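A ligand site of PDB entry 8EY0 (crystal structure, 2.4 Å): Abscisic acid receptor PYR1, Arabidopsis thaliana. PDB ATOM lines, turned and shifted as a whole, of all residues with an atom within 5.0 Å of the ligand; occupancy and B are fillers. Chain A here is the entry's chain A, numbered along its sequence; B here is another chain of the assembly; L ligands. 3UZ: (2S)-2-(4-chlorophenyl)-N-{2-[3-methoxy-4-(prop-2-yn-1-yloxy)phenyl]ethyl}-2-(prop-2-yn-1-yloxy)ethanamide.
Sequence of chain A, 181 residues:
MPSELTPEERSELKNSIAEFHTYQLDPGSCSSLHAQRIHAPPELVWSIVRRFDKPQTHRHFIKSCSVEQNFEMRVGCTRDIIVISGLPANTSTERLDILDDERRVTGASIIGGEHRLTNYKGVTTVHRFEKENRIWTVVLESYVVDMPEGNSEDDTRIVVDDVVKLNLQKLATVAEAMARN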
ATOM      1  N   ARG A  59     -36.236  23.237 -11.742  1.00  0.00           N
ATOM      2  CA  ARG A  59     -34.963  23.578 -12.353  1.00  0.00           C
ATOM      3  C   ARG A  59     -33.883  23.708 -11.286  1.00  0.00           C
ATOM      4  O   ARG A  59     -34.169  23.905 -10.103  1.00  0.00           O
ATOM      5  CB  ARG A  59     -35.065  24.876 -13.168  1.00  0.00           C
ATOM      6  CG  ARG A  59     -36.074  24.766 -14.325  1.00  0.00           C
ATOM      7  CD  ARG A  59     -36.104  26.015 -15.193  1.00  0.00           C
ATOM      8  NE  ARG A  59     -35.063  26.057 -16.208  1.00  0.00           N
ATOM      9  CZ  ARG A  59     -35.047  25.301 -17.306  1.00  0.00           C
ATOM     10  NH1 ARG A  59     -35.999  24.402 -17.517  1.00  0.00           N
ATOM     11  NH2 ARG A  59     -34.053  25.436 -18.183  1.00  0.00           N
ATOM     12  N   HIS A  60     -32.632  23.596 -11.732  1.00  0.00           N
ATOM     13  CA  HIS A  60     -31.493  23.570 -10.835  1.00  0.00           C
ATOM     14  C   HIS A  60     -30.909  24.963 -10.650  1.00  0.00           C
ATOM     15  O   HIS A  60     -31.250  25.908 -11.363  1.00  0.00           O
ATOM     16  CB  HIS A  60     -30.411  22.618 -11.378  1.00  0.00           C
ATOM     17  CG  HIS A  60     -30.616  21.176 -10.987  1.00  0.00           C
ATOM     18  ND1 HIS A  60     -31.008  20.208 -11.886  1.00  0.00           N
ATOM     19  CD2 HIS A  60     -30.423  20.549  -9.808  1.00  0.00           C
ATOM     20  CE1 HIS A  60     -31.078  19.050 -11.272  1.00  0.00           C
ATOM     21  NE2 HIS A  60     -30.732  19.217 -10.007  1.00  0.00           N
ATOM     22  N   PHE A  61     -30.031  25.094  -9.640  1.00  0.00           N
ATOM     23  CA  PHE A  61     -29.098  26.203  -9.514  1.00  0.00           C
ATOM     24  C   PHE A  61     -29.757  27.503  -9.069  1.00  0.00           C
ATOM     25  O   PHE A  61     -29.168  28.579  -9.239  1.00  0.00           O
ATOM     26  CB  PHE A  61     -28.345  26.457 -10.827  1.00  0.00           C
ATOM     27  CG  PHE A  61     -27.851  25.210 -11.512  1.00  0.00           C
ATOM     28  CD1 PHE A  61     -28.289  24.898 -12.793  1.00  0.00           C
ATOM     29  CD2 PHE A  61     -26.946  24.357 -10.883  1.00  0.00           C
ATOM     30  CE1 PHE A  61     -27.843  23.752 -13.435  1.00  0.00           C
ATOM     31  CE2 PHE A  61     -26.494  23.199 -11.520  1.00  0.00           C
ATOM     32  CZ  PHE A  61     -26.945  22.899 -12.794  1.00  0.00           C
ATOM     33  N   ILE A  62     -30.960  27.443  -8.519  1.00  0.00           N
ATOM     34  CA  ILE A  62     -31.681  28.632  -8.087  1.00  0.00           C
ATOM     35  C   ILE A  62     -31.607  28.705  -6.559  1.00  0.00           C
ATOM     36  O   ILE A  62     -32.168  27.861  -5.855  1.00  0.00           O
ATOM     37  CB  ILE A  62     -33.135  28.604  -8.573  1.00  0.00           C
ATOM     38  CG1 ILE A  62     -33.145  28.655 -10.103  1.00  0.00           C
ATOM     39  CG2 ILE A  62     -33.931  29.729  -7.910  1.00  0.00           C
ATOM     40  CD1 ILE A  62     -34.467  28.264 -10.740  1.00  0.00           C
ATOM     41  N   ARG A  79     -39.005  37.654 -13.657  1.00  0.00           N
ATOM     42  CA  ARG A  79     -38.551  37.092 -12.391  1.00  0.00           C
ATOM     43  C   ARG A  79     -37.076  37.402 -12.220  1.00  0.00           C
ATOM     44  O   ARG A  79     -36.319  37.499 -13.187  1.00  0.00           O
ATOM     45  CB  ARG A  79     -38.796  35.578 -12.330  1.00  0.00           C
ATOM     46  CG  ARG A  79     -38.008  34.772 -13.345  1.00  0.00           C
ATOM     47  CD  ARG A  79     -38.429  33.298 -13.361  1.00  0.00           C
ATOM     48  NE  ARG A  79     -37.700  32.565 -14.392  1.00  0.00           N
ATOM     49  CZ  ARG A  79     -38.141  31.460 -14.997  1.00  0.00           C
ATOM     50  NH1 ARG A  79     -37.401  30.899 -15.938  1.00  0.00           N
ATOM     51  NH2 ARG A  79     -39.326  30.930 -14.690  1.00  0.00           N
ATOM     52  N   ILE A  81     -33.748  36.031 -10.345  1.00  0.00           N
ATOM     53  CA  ILE A  81     -33.186  34.833  -9.744  1.00  0.00           C
ATOM     54  C   ILE A  81     -31.815  35.147  -9.182  1.00  0.00           C
ATOM     55  O   ILE A  81     -30.977  35.767  -9.859  1.00  0.00           O
ATOM     56  CB  ILE A  81     -33.113  33.684 -10.762  1.00  0.00           C
ATOM     57  CG1 ILE A  81     -34.530  33.171 -11.027  1.00  0.00           C
ATOM     58  CG2 ILE A  81     -32.128  32.581 -10.271  1.00  0.00           C
ATOM     59  CD1 ILE A  81     -34.606  32.165 -12.130  1.00  0.00           C
ATOM     60  N   VAL A  83     -28.596  33.013  -8.337  1.00  0.00           N
ATOM     61  CA  VAL A  83     -28.054  31.688  -8.639  1.00  0.00           C
ATOM     62  C   VAL A  83     -27.252  31.166  -7.456  1.00  0.00           C
ATOM     63  O   VAL A  83     -26.647  31.947  -6.709  1.00  0.00           O
ATOM     64  CB  VAL A  83     -27.191  31.802  -9.918  1.00  0.00           C
ATOM     65  CG1 VAL A  83     -26.595  30.435 -10.320  1.00  0.00           C
ATOM     66  CG2 VAL A  83     -28.019  32.423 -11.045  1.00  0.00           C
ATOM     67  N   LEU A  87     -20.965  29.072  -9.774  1.00  0.00           N
ATOM     68  CA  LEU A  87     -21.308  29.017 -11.193  1.00  0.00           C
ATOM     69  C   LEU A  87     -20.857  30.295 -11.902  1.00  0.00           C
ATOM     70  O   LEU A  87     -20.608  31.322 -11.261  1.00  0.00           O
ATOM     71  CB  LEU A  87     -22.825  28.831 -11.378  1.00  0.00           C
ATOM     72  CG  LEU A  87     -23.324  27.424 -11.030  1.00  0.00           C
ATOM     73  CD1 LEU A  87     -24.818  27.393 -10.888  1.00  0.00           C
ATOM     74  CD2 LEU A  87     -22.907  26.414 -12.084  1.00  0.00           C
ATOM     75  N   PRO A  88     -20.723  30.253 -13.224  1.00  0.00           N
ATOM     76  CA  PRO A  88     -20.366  31.473 -13.960  1.00  0.00           C
ATOM     77  C   PRO A  88     -21.577  32.370 -14.216  1.00  0.00           C
ATOM     78  O   PRO A  88     -21.613  33.130 -15.181  1.00  0.00           O
ATOM     79  CB  PRO A  88     -19.779  30.926 -15.267  1.00  0.00           C
ATOM     80  CG  PRO A  88     -20.574  29.643 -15.493  1.00  0.00           C
ATOM     81  CD  PRO A  88     -20.753  29.068 -14.106  1.00  0.00           C
ATOM     82  N   ALA A  89     -22.577  32.265 -13.342  1.00  0.00           N
ATOM     83  CA  ALA A  89     -23.692  33.198 -13.288  1.00  0.00           C
ATOM     84  C   ALA A  89     -24.014  33.450 -11.833  1.00  0.00           C
ATOM     85  O   ALA A  89     -24.056  32.524 -11.010  1.00  0.00           O
ATOM     86  CB  ALA A  89     -24.940  32.654 -13.992  1.00  0.00           C
ATOM     87  N   THR A  91     -26.665  36.115 -11.136  1.00  0.00           N
ATOM     88  CA  THR A  91     -28.061  36.487 -11.174  1.00  0.00           C
ATOM     89  C   THR A  91     -28.597  36.304 -12.583  1.00  0.00           C
ATOM     90  O   THR A  91     -27.838  36.297 -13.564  1.00  0.00           O
ATOM     91  CB  THR A  91     -28.250  37.941 -10.740  1.00  0.00           C
ATOM     92  OG1 THR A  91     -27.500  38.766 -11.624  1.00  0.00           O
ATOM     93  CG2 THR A  91     -27.764  38.172  -9.289  1.00  0.00           C
ATOM     94  N   SER A  92     -29.911  36.169 -12.684  1.00  0.00           N
ATOM     95  CA  SER A  92     -30.569  36.083 -13.972  1.00  0.00           C
ATOM     96  C   SER A  92     -31.891  36.807 -13.882  1.00  0.00           C
ATOM     97  O   SER A  92     -32.674  36.562 -12.963  1.00  0.00           O
ATOM     98  CB  SER A  92     -30.787  34.628 -14.388  1.00  0.00           C
ATOM     99  OG  SER A  92     -31.127  34.550 -15.762  1.00  0.00           O
ATOM    100  N   GLU A  94     -35.329  37.124 -15.954  1.00  0.00           N
ATOM    101  CA  GLU A  94     -35.982  36.316 -16.962  1.00  0.00           C
ATOM    102  C   GLU A  94     -37.383  36.860 -17.211  1.00  0.00           C
ATOM    103  O   GLU A  94     -37.992  37.508 -16.354  1.00  0.00           O
ATOM    104  CB  GLU A  94     -35.992  34.841 -16.550  1.00  0.00           C
ATOM    105  CG  GLU A  94     -34.609  34.196 -16.762  1.00  0.00           C
ATOM    106  CD  GLU A  94     -34.329  32.986 -15.889  1.00  0.00           C
ATOM    107  OE1 GLU A  94     -35.286  32.449 -15.277  1.00  0.00           O
ATOM    108  OE2 GLU A  94     -33.150  32.573 -15.817  1.00  0.00           O
ATOM    109  N   ALA A 108     -39.620  31.564 -22.475  1.00  0.00           N
ATOM    110  CA  ALA A 108     -39.053  32.623 -21.665  1.00  0.00           C
ATOM    111  C   ALA A 108     -37.726  33.087 -22.242  1.00  0.00           C
ATOM    112  O   ALA A 108     -37.020  32.332 -22.930  1.00  0.00           O
ATOM    113  CB  ALA A 108     -38.867  32.183 -20.215  1.00  0.00           C
ATOM    114  N   SER A 109     -37.391  34.348 -21.957  1.00  0.00           N
ATOM    115  CA  SER A 109     -36.144  34.975 -22.360  1.00  0.00           C
ATOM    116  C   SER A 109     -35.329  35.366 -21.143  1.00  0.00           C
ATOM    117  O   SER A 109     -35.862  35.601 -20.058  1.00  0.00           O
ATOM    118  CB  SER A 109     -36.388  36.230 -23.210  1.00  0.00           C
ATOM    119  OG  SER A 109     -36.666  35.904 -24.546  1.00  0.00           O
ATOM    120  N   ILE A 110     -34.014  35.431 -21.329  1.00  0.00           N
ATOM    121  CA  ILE A 110     -33.114  35.965 -20.321  1.00  0.00           C
ATOM    122  C   ILE A 110     -32.736  37.375 -20.767  1.00  0.00           C
ATOM    123  O   ILE A 110     -32.070  37.542 -21.805  1.00  0.00           O
ATOM    124  CB  ILE A 110     -31.877  35.073 -20.133  1.00  0.00           C
ATOM    125  CG1 ILE A 110     -32.293  33.687 -19.612  1.00  0.00           C
ATOM    126  CG2 ILE A 110     -30.898  35.761 -19.204  1.00  0.00           C
ATOM    127  CD1 ILE A 110     -31.165  32.681 -19.494  1.00  0.00           C
ATOM    128  N   HIS A 115     -24.077  37.189 -16.044  1.00  0.00           N
ATOM    129  CA  HIS A 115     -23.784  35.894 -16.648  1.00  0.00           C
ATOM    130  C   HIS A 115     -23.340  36.178 -18.084  1.00  0.00           C
ATOM    131  O   HIS A 115     -23.249  37.337 -18.495  1.00  0.00           O
ATOM    132  CB  HIS A 115     -24.982  34.969 -16.581  1.00  0.00           C
ATOM    133  CG  HIS A 115     -26.207  35.545 -17.223  1.00  0.00           C
ATOM    134  ND1 HIS A 115     -26.395  35.539 -18.590  1.00  0.00           N
ATOM    135  CD2 HIS A 115     -27.270  36.183 -16.695  1.00  0.00           C
ATOM    136  CE1 HIS A 115     -27.543  36.127 -18.866  1.00  0.00           C
ATOM    137  NE2 HIS A 115     -28.092  36.530 -17.734  1.00  0.00           N
ATOM    138  N   LEU A 117     -24.804  34.831 -21.052  1.00  0.00           N
ATOM    139  CA  LEU A 117     -25.801  34.382 -22.033  1.00  0.00           C
ATOM    140  C   LEU A 117     -26.527  35.605 -22.583  1.00  0.00           C
ATOM    141  O   LEU A 117     -27.384  36.189 -21.899  1.00  0.00           O
ATOM    142  CB  LEU A 117     -26.790  33.390 -21.433  1.00  0.00           C
ATOM    143  CG  LEU A 117     -26.281  32.124 -20.738  1.00  0.00           C
ATOM    144  CD1 LEU A 117     -27.456  31.339 -20.155  1.00  0.00           C
ATOM    145  CD2 LEU A 117     -25.519  31.284 -21.718  1.00  0.00           C
ATOM    146  N   TYR A 120     -30.600  34.721 -25.091  1.00  0.00           N
ATOM    147  CA  TYR A 120     -31.180  33.418 -24.824  1.00  0.00           C
ATOM    148  C   TYR A 120     -32.710  33.520 -24.887  1.00  0.00           C
ATOM    149  O   TYR A 120     -33.297  34.409 -24.275  1.00  0.00           O
ATOM    150  CB  TYR A 120     -30.739  32.878 -23.456  1.00  0.00           C
ATOM    151  CG  TYR A 120     -31.276  31.497 -23.143  1.00  0.00           C
ATOM    152  CD1 TYR A 120     -30.458  30.367 -23.273  1.00  0.00           C
ATOM    153  CD2 TYR A 120     -32.605  31.302 -22.743  1.00  0.00           C
ATOM    154  CE1 TYR A 120     -30.952  29.088 -22.992  1.00  0.00           C
ATOM    155  CE2 TYR A 120     -33.099  30.023 -22.462  1.00  0.00           C
ATOM    156  CZ  TYR A 120     -32.279  28.928 -22.591  1.00  0.00           C
ATOM    157  OH  TYR A 120     -32.770  27.677 -22.326  1.00  0.00           O
ATOM    158  N   VAL A 159     -22.172  23.295 -22.727  1.00  0.00           N
ATOM    159  CA  VAL A 159     -22.560  23.919 -21.467  1.00  0.00           C
ATOM    160  C   VAL A 159     -24.083  24.005 -21.329  1.00  0.00           C
ATOM    161  O   VAL A 159     -24.646  23.659 -20.287  1.00  0.00           O
ATOM    162  CB  VAL A 159     -21.916  25.310 -21.352  1.00  0.00           C
ATOM    163  CG1 VAL A 159     -22.517  26.085 -20.177  1.00  0.00           C
ATOM    164  CG2 VAL A 159     -20.400  25.195 -21.187  1.00  0.00           C
ATOM    165  N   VAL A 160     -24.762  24.483 -22.370  1.00  0.00           N
ATOM    166  CA  VAL A 160     -26.202  24.739 -22.273  1.00  0.00           C
ATOM    167  C   VAL A 160     -27.002  23.455 -22.426  1.00  0.00           C
ATOM    168  O   VAL A 160     -28.060  23.299 -21.794  1.00  0.00           O
ATOM    169  CB  VAL A 160     -26.623  25.809 -23.288  1.00  0.00           C
ATOM    170  CG1 VAL A 160     -28.137  26.030 -23.275  1.00  0.00           C
ATOM    171  CG2 VAL A 160     -25.923  27.108 -22.999  1.00  0.00           C
ATOM    172  N   VAL A 163     -27.251  21.862 -18.881  1.00  0.00           N
ATOM    173  CA  VAL A 163     -28.217  22.523 -17.990  1.00  0.00           C
ATOM    174  C   VAL A 163     -29.641  22.116 -18.364  1.00  0.00           C
ATOM    175  O   VAL A 163     -30.442  21.728 -17.514  1.00  0.00           O
ATOM    176  CB  VAL A 163     -28.050  24.053 -18.035  1.00  0.00           C
ATOM    177  CG1 VAL A 163     -29.175  24.726 -17.302  1.00  0.00           C
ATOM    178  CG2 VAL A 163     -26.704  24.455 -17.449  1.00  0.00           C
ATOM    179  N   VAL A 164     -29.971  22.197 -19.657  1.00  0.00           N
ATOM    180  CA  VAL A 164     -31.311  21.827 -20.095  1.00  0.00           C
ATOM    181  C   VAL A 164     -31.598  20.357 -19.783  1.00  0.00           C
ATOM    182  O   VAL A 164     -32.673  20.002 -19.286  1.00  0.00           O
ATOM    183  CB  VAL A 164     -31.509  22.148 -21.585  1.00  0.00           C
ATOM    184  CG1 VAL A 164     -32.735  21.415 -22.126  1.00  0.00           C
ATOM    185  CG2 VAL A 164     -31.654  23.651 -21.769  1.00  0.00           C
ATOM    186  N   ASN A 167     -32.134  19.910 -16.101  1.00  0.00           N
ATOM    187  CA  ASN A 167     -33.417  20.488 -15.728  1.00  0.00           C
ATOM    188  C   ASN A 167     -34.586  19.617 -16.177  1.00  0.00           C
ATOM    189  O   ASN A 167     -35.642  19.623 -15.539  1.00  0.00           O
ATOM    190  CB  ASN A 167     -33.522  21.903 -16.283  1.00  0.00           C
ATOM    191  CG  ASN A 167     -32.658  22.889 -15.521  1.00  0.00           C
ATOM    192  OD1 ASN A 167     -31.981  22.529 -14.569  1.00  0.00           O
ATOM    193  ND2 ASN A 167     -32.675  24.141 -15.938  1.00  0.00           N
ATOM    194  N   GLY B 214     -18.612  23.494 -17.853  1.00  0.00           N
ATOM    195  CA  GLY B 214     -18.943  24.905 -17.777  1.00  0.00           C
ATOM    196  C   GLY B 214     -19.494  25.362 -16.444  1.00  0.00           C
ATOM    197  O   GLY B 214     -20.004  26.482 -16.364  1.00  0.00           O
ATOM    198  N   ARG B 215     -19.402  24.535 -15.398  1.00  0.00           N
ATOM    199  CA  ARG B 215     -20.021  24.864 -14.117  1.00  0.00           C
ATOM    200  C   ARG B 215     -19.006  24.939 -12.973  1.00  0.00           C
ATOM    201  O   ARG B 215     -18.661  26.040 -12.541  1.00  0.00           O
ATOM    202  CB  ARG B 215     -21.128  23.843 -13.799  1.00  0.00           C
ATOM    203  CG  ARG B 215     -22.256  23.872 -14.868  1.00  0.00           C
ATOM    204  CD  ARG B 215     -23.551  23.245 -14.369  1.00  0.00           C
ATOM    205  NE  ARG B 215     -23.351  21.868 -13.938  1.00  0.00           N
ATOM    206  CZ  ARG B 215     -23.399  20.821 -14.758  1.00  0.00           C
ATOM    207  NH1 ARG B 215     -23.645  20.996 -16.048  1.00  0.00           N
ATOM    208  NH2 ARG B 215     -23.201  19.587 -14.271  1.00  0.00           N
HETATM  209  CAC 3UZ L   1     -31.363  27.545 -19.215  1.00  0.00           C
HETATM  210  CAB 3UZ L   1     -30.070  27.309 -19.649  1.00  0.00           C
HETATM  211  CAA 3UZ L   1     -29.000  27.910 -18.997  1.00  0.00           C
HETATM  212 CL1  3UZ L   1     -27.429  27.625 -19.498  1.00  0.00          CL
HETATM  213  CAF 3UZ L   1     -29.202  28.752 -17.906  1.00  0.00           C
HETATM  214  CAE 3UZ L   1     -30.502  28.983 -17.477  1.00  0.00           C
HETATM  215  CAD 3UZ L   1     -31.586  28.394 -18.122  1.00  0.00           C
HETATM  216  CAH 3UZ L   1     -32.883  28.595 -17.640  1.00  0.00           C
HETATM  217  OAI 3UZ L   1     -33.446  29.768 -18.123  1.00  0.00           O
HETATM  218  CAJ 3UZ L   1     -34.748  29.413 -18.595  1.00  0.00           C
HETATM  219  CAK 3UZ L   1     -35.455  30.652 -18.783  1.00  0.00           C
HETATM  220  CAL 3UZ L   1     -35.958  31.648 -18.917  1.00  0.00           C
HETATM  221  CAM 3UZ L   1     -32.867  28.538 -16.089  1.00  0.00           C
HETATM  222  OAN 3UZ L   1     -33.090  27.459 -15.546  1.00  0.00           O
HETATM  223  NAO 3UZ L   1     -32.558  29.671 -15.402  1.00  0.00           N
HETATM  224  CAP 3UZ L   1     -32.462  29.686 -13.926  1.00  0.00           C
HETATM  225  CAQ 3UZ L   1     -31.343  30.628 -13.417  1.00  0.00           C
HETATM  226  CAR 3UZ L   1     -30.073  30.214 -13.871  1.00  0.00           C
HETATM  227  CAW 3UZ L   1     -29.285  31.064 -14.670  1.00  0.00           C
HETATM  228  CAV 3UZ L   1     -28.036  30.645 -15.130  1.00  0.00           C
HETATM  229  OAX 3UZ L   1     -27.203  31.424 -15.915  1.00  0.00           O
HETATM  230  CAY 3UZ L   1     -27.827  32.494 -16.641  1.00  0.00           C
HETATM  231  CAS 3UZ L   1     -29.582  28.932 -13.562  1.00  0.00           C
HETATM  232  CAT 3UZ L   1     -28.335  28.508 -14.014  1.00  0.00           C
HETATM  233  CAU 3UZ L   1     -27.568  29.371 -14.794  1.00  0.00           C
HETATM  234  OAZ 3UZ L   1     -26.320  29.039 -15.289  1.00  0.00           O
HETATM  235  CBA 3UZ L   1     -26.025  27.642 -15.346  1.00  0.00           C
HETATM  236  CBB 3UZ L   1     -24.658  27.490 -15.859  1.00  0.00           C
HETATM  237  CBC 3UZ L   1     -23.492  27.394 -16.303  1.00  0.00           C
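NE of Arg 59 sits at hydrogen-bond distance from OAN of the ligand, 2.5 Å away. OE2 of Glu 94 is in hydrogen-bond range of NAO of the ligand. The side-chain amide nitrogen (ND2) of Asn 167 lies within hydrogen-bond range of an oxygen (OAN) of the ligand, at 3.4 Å.
Residues that only touch the ligand: Phe 61 (3.8 Å), Arg 79 (3.4 Å), Ile 81 (3.7 Å), Pro 88 (3.8 Å), Ala 89 (3.2 Å), Ser 92 (3.9 Å), Ala 108 (3.2 Å), Ile 110 (3.9 Å), His 115 (3.5 Å), Leu 117 (3.7 Å), Tyr 120 (3.4 Å), Val 160 (3.8 Å), Val 163 (3.6 Å), Gly 214 of chain B (3.6 Å) and Arg 215 of chain B (3.999 Å). Hydrophobic or aromatic side chains that line the ligand: Phe 61, Ile 81, Pro 88, Ala 89, Ala 108, Ile 110, His 115, Leu 117, Tyr 120, Val 160 and Val 163.
The guanidinium group of Arg 59 sits close to the side-chain amide nitrogen of Asn 167 (2.9 Å). The side-chain carboxylate (OE1) of Glu 94 lies within salt-bridge range of the guanidinium group (NE) of Arg 79, at 2.6 Å. OE2 of Glu 94 lies within hydrogen-bond range of OG of Ser 92 (2.8 Å). O of Val 163 lies close to OD1 of Asn 167 (3.4 Å). The backbone NH (N) of His 60 lies within hydrogen-bond range of the side-chain amide oxygen (OD1) of Asn 167 (3.1 Å). The backbone carbonyl oxygen (O) of Tyr 120 lies within hydrogen-bond range of the backbone NH (N) of Ile 110 (3.2 Å). A ring nitrogen (ND1) of His 115 is in hydrogen-bond range of the backbone NH of Leu 117 (3.0 Å). The backbone NH (N) of Ile 81 is in hydrogen-bond range of the backbone carbonyl oxygen (O) of Ser 92.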
